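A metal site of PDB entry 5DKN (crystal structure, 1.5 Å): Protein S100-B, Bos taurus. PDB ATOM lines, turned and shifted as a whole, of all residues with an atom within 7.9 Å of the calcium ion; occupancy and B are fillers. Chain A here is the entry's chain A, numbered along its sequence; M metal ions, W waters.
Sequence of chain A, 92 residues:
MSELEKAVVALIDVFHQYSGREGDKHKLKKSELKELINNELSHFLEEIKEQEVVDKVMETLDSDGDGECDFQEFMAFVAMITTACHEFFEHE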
ATOM      1  N   LYS A  27      15.548 -16.218 -15.312  1.00  0.00           N
ATOM      2  CA  LYS A  27      14.674 -15.282 -15.993  1.00  0.00           C
ATOM      3  C   LYS A  27      15.450 -14.435 -16.992  1.00  0.00           C
ATOM      4  O   LYS A  27      16.641 -14.186 -16.805  1.00  0.00           O
ATOM      5  CB  LYS A  27      13.961 -14.365 -14.984  1.00  0.00           C
ATOM      6  CG  LYS A  27      13.165 -15.066 -13.892  1.00  0.00           C
ATOM      7  CD  LYS A  27      12.520 -14.058 -12.959  1.00  0.00           C
ATOM      8  CE  LYS A  27      11.802 -14.747 -11.815  1.00  0.00           C
ATOM      9  NZ  LYS A  27      11.281 -13.765 -10.818  1.00  0.00           N
ATOM     10  N   LEU A  28      14.762 -14.002 -18.049  1.00  0.00           N
ATOM     11  CA  LEU A  28      15.305 -13.042 -18.983  1.00  0.00           C
ATOM     12  C   LEU A  28      14.929 -11.618 -18.554  1.00  0.00           C
ATOM     13  O   LEU A  28      13.741 -11.273 -18.534  1.00  0.00           O
ATOM     14  CB  LEU A  28      14.748 -13.278 -20.388  1.00  0.00           C
ATOM     15  CG  LEU A  28      14.978 -14.627 -21.057  1.00  0.00           C
ATOM     16  CD1 LEU A  28      13.980 -14.785 -22.216  1.00  0.00           C
ATOM     17  CD2 LEU A  28      16.407 -14.736 -21.559  1.00  0.00           C
ATOM     18  N   MET A  58       8.633  -6.648 -23.515  1.00  0.00           N
ATOM     19  CA  MET A  58       8.577  -7.132 -22.138  1.00  0.00           C
ATOM     20  C   MET A  58       7.223  -6.841 -21.483  1.00  0.00           C
ATOM     21  O   MET A  58       6.719  -7.661 -20.716  1.00  0.00           O
ATOM     22  CB  MET A  58       9.718  -6.552 -21.293  1.00  0.00           C
ATOM     23  CG  MET A  58       9.813  -7.162 -19.890  1.00  0.00           C
ATOM     24  SD  MET A  58      10.156  -8.945 -19.890  1.00  0.00           S
ATOM     25  CE  MET A  58      11.937  -8.906 -20.136  1.00  0.00           C
ATOM     26  N   LEU A  61       5.022  -9.577 -22.624  1.00  0.00           N
ATOM     27  CA  LEU A  61       5.385 -10.921 -22.145  1.00  0.00           C
ATOM     28  C   LEU A  61       5.320 -11.106 -20.635  1.00  0.00           C
ATOM     29  O   LEU A  61       5.153 -12.229 -20.143  1.00  0.00           O
ATOM     30  CB  LEU A  61       6.782 -11.311 -22.624  1.00  0.00           C
ATOM     31  CG  LEU A  61       7.009 -11.351 -24.127  1.00  0.00           C
ATOM     32  CD1 LEU A  61       8.399 -11.882 -24.446  1.00  0.00           C
ATOM     33  CD2 LEU A  61       5.935 -12.206 -24.781  1.00  0.00           C
ATOM     34  N   ASP A  62       5.456 -10.014 -19.883  1.00  0.00           N
ATOM     35  CA  ASP A  62       5.587 -10.106 -18.427  1.00  0.00           C
ATOM     36  C   ASP A  62       4.220 -10.137 -17.746  1.00  0.00           C
ATOM     37  O   ASP A  62       3.622  -9.099 -17.468  1.00  0.00           O
ATOM     38  CB  ASP A  62       6.428  -8.934 -17.895  1.00  0.00           C
ATOM     39  CG  ASP A  62       6.562  -8.955 -16.390  1.00  0.00           C
ATOM     40  OD1 ASP A  62       6.502 -10.039 -15.785  1.00  0.00           O
ATOM     41  OD2 ASP A  62       6.713  -7.868 -15.788  1.00  0.00           O
ATOM     42  N   SER A  63       3.728 -11.341 -17.463  1.00  0.00           N
ATOM     43  CA  SER A  63       2.389 -11.507 -16.900  1.00  0.00           C
ATOM     44  C   SER A  63       2.328 -11.412 -15.373  1.00  0.00           C
ATOM     45  O   SER A  63       1.226 -11.322 -14.828  1.00  0.00           O
ATOM     46  CB  SER A  63       1.784 -12.820 -17.365  1.00  0.00           C
ATOM     47  OG  SER A  63       1.663 -12.864 -18.775  1.00  0.00           O
ATOM     48  N   ASP A  64       3.459 -11.459 -14.680  1.00  0.00           N
ATOM     49  CA  ASP A  64       3.420 -11.353 -13.223  1.00  0.00           C
ATOM     50  C   ASP A  64       4.060 -10.077 -12.669  1.00  0.00           C
ATOM     51  O   ASP A  64       4.275  -9.960 -11.471  1.00  0.00           O
ATOM     52  CB  ASP A  64       3.973 -12.614 -12.516  1.00  0.00           C
ATOM     53  CG  ASP A  64       5.460 -12.835 -12.772  1.00  0.00           C
ATOM     54  OD1 ASP A  64       6.084 -12.072 -13.539  1.00  0.00           O
ATOM     55  OD2 ASP A  64       6.007 -13.799 -12.181  1.00  0.00           O
ATOM     56  N   GLY A  65       4.370  -9.147 -13.570  1.00  0.00           N
ATOM     57  CA  GLY A  65       4.776  -7.805 -13.172  1.00  0.00           C
ATOM     58  C   GLY A  65       6.141  -7.675 -12.525  1.00  0.00           C
ATOM     59  O   GLY A  65       6.419  -6.662 -11.872  1.00  0.00           O
ATOM     60  N   ASP A  66       7.007  -8.672 -12.700  1.00  0.00           N
ATOM     61  CA  ASP A  66       8.333  -8.580 -12.097  1.00  0.00           C
ATOM     62  C   ASP A  66       9.380  -7.945 -13.019  1.00  0.00           C
ATOM     63  O   ASP A  66      10.539  -7.791 -12.635  1.00  0.00           O
ATOM     64  CB  ASP A  66       8.804  -9.942 -11.555  1.00  0.00           C
ATOM     65  CG  ASP A  66       9.174 -10.934 -12.656  1.00  0.00           C
ATOM     66  OD1 ASP A  66       8.849 -10.700 -13.838  1.00  0.00           O
ATOM     67  OD2 ASP A  66       9.774 -11.973 -12.325  1.00  0.00           O
ATOM     68  N   GLY A  67       8.946  -7.566 -14.222  1.00  0.00           N
ATOM     69  CA  GLY A  67       9.802  -6.865 -15.160  1.00  0.00           C
ATOM     70  C   GLY A  67      10.703  -7.762 -15.978  1.00  0.00           C
ATOM     71  O   GLY A  67      11.530  -7.277 -16.774  1.00  0.00           O
ATOM     72  N   GLU A  68      10.545  -9.074 -15.794  1.00  0.00           N
ATOM     73  CA  GLU A  68      11.361 -10.073 -16.458  1.00  0.00           C
ATOM     74  C   GLU A  68      10.483 -11.145 -17.075  1.00  0.00           C
ATOM     75  O   GLU A  68       9.305 -11.264 -16.758  1.00  0.00           O
ATOM     76  CB  GLU A  68      12.355 -10.695 -15.479  1.00  0.00           C
ATOM     77  CG  GLU A  68      13.262  -9.673 -14.797  1.00  0.00           C
ATOM     78  CD  GLU A  68      14.592 -10.247 -14.351  1.00  0.00           C
ATOM     79  OE1 GLU A  68      15.020 -11.256 -14.937  1.00  0.00           O
ATOM     80  OE2 GLU A  68      15.207  -9.673 -13.417  1.00  0.00           O
ATOM     81  N   CYS A  69      11.080 -11.925 -17.974  1.00  0.00           N
ATOM     82  CA  CYS A  69      10.396 -13.011 -18.623  1.00  0.00           C
ATOM     83  C   CYS A  69      10.906 -14.360 -18.089  1.00  0.00           C
ATOM     84  O   CYS A  69      12.037 -14.758 -18.382  1.00  0.00           O
ATOM     85  CB  CYS A  69      10.593 -12.912 -20.135  1.00  0.00           C
ATOM     86  SG  CYS A  69       9.805 -14.212 -21.103  1.00  0.00           S
ATOM     87  N   ASP A  70      10.074 -15.048 -17.314  1.00  0.00           N
ATOM     88  CA  ASP A  70      10.447 -16.363 -16.788  1.00  0.00           C
ATOM     89  C   ASP A  70      10.204 -17.478 -17.813  1.00  0.00           C
ATOM     90  O   ASP A  70       9.854 -17.184 -18.967  1.00  0.00           O
ATOM     91  CB  ASP A  70       9.789 -16.648 -15.420  1.00  0.00           C
ATOM     92  CG  ASP A  70       8.265 -16.798 -15.487  1.00  0.00           C
ATOM     93  OD1 ASP A  70       7.721 -17.028 -16.582  1.00  0.00           O
ATOM     94  OD2 ASP A  70       7.616 -16.739 -14.409  1.00  0.00           O
ATOM     95  N   PHE A  71      10.402 -18.739 -17.433  1.00  0.00           N
ATOM     96  CA  PHE A  71      10.271 -19.803 -18.428  1.00  0.00           C
ATOM     97  C   PHE A  71       8.845 -19.923 -18.968  1.00  0.00           C
ATOM     98  O   PHE A  71       8.670 -20.067 -20.183  1.00  0.00           O
ATOM     99  CB  PHE A  71      10.757 -21.148 -17.891  1.00  0.00           C
ATOM    100  CG  PHE A  71      10.869 -22.205 -18.942  1.00  0.00           C
ATOM    101  CD1 PHE A  71      11.956 -22.236 -19.794  1.00  0.00           C
ATOM    102  CD2 PHE A  71       9.867 -23.162 -19.108  1.00  0.00           C
ATOM    103  CE1 PHE A  71      12.060 -23.208 -20.785  1.00  0.00           C
ATOM    104  CE2 PHE A  71       9.968 -24.124 -20.095  1.00  0.00           C
ATOM    105  CZ  PHE A  71      11.063 -24.150 -20.928  1.00  0.00           C
ATOM    106  N   GLU A  73       6.556 -17.600 -19.139  1.00  0.00           N
ATOM    107  CA  GLU A  73       6.331 -16.455 -20.014  1.00  0.00           C
ATOM    108  C   GLU A  73       7.067 -16.612 -21.353  1.00  0.00           C
ATOM    109  O   GLU A  73       6.577 -16.193 -22.409  1.00  0.00           O
ATOM    110  CB  GLU A  73       6.723 -15.164 -19.291  1.00  0.00           C
ATOM    111  CG  GLU A  73       5.817 -14.884 -18.073  1.00  0.00           C
ATOM    112  CD  GLU A  73       6.401 -13.855 -17.109  1.00  0.00           C
ATOM    113  OE1 GLU A  73       7.630 -13.662 -17.097  1.00  0.00           O
ATOM    114  OE2 GLU A  73       5.627 -13.239 -16.335  1.00  0.00           O
HETATM  115 CA    CA M   1       7.579 -12.011 -15.309  1.00  0.00          CA
HETATM  116  O   HOH W   1       8.692 -13.727 -14.065  1.00  0.00           O
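N of Gly 65 sits close to OD2 of Asp 62 (3.5 Å). The side-chain carboxylate (OD2) of Asp 62 lies within hydrogen-bond range of the backbone NH (N) of Gly 67, 2.7 Å away. NZ of Lys 27 lies within salt-bridge range of OD2 of Asp 66, 2.8 Å away. The backbone NH (N) of Glu 73 sits at hydrogen-bond distance from the side-chain carboxylate (OD1) of Asp 70. The side-chain carboxylate of Glu 73 lies close to the backbone NH of Ser 63 (2.9 Å).
Of the 15 residues printed, 5 come within 4 Å of the calcium ion.
OD1 of Asp 62 binds the calcium ion (2.3 Å). The side-chain carboxylate (OD1) of Asp 64 is bound to the calcium ion (2.3 Å). The side-chain carboxylate (OD1) of Asp 66 binds the calcium ion, at 2.3 Å. The backbone carbonyl oxygen (O) of Glu 68 is bound to the calcium ion (2.4 Å). Water W1 binds the calcium ion, at 2.4 Å. The calcium ion is bound by the side-chain carboxylate (OE1) of Glu 73, 2.4 Å away. The calcium ion is bound by the side-chain carboxylate (OE2) of Glu 73 (2.5 Å).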
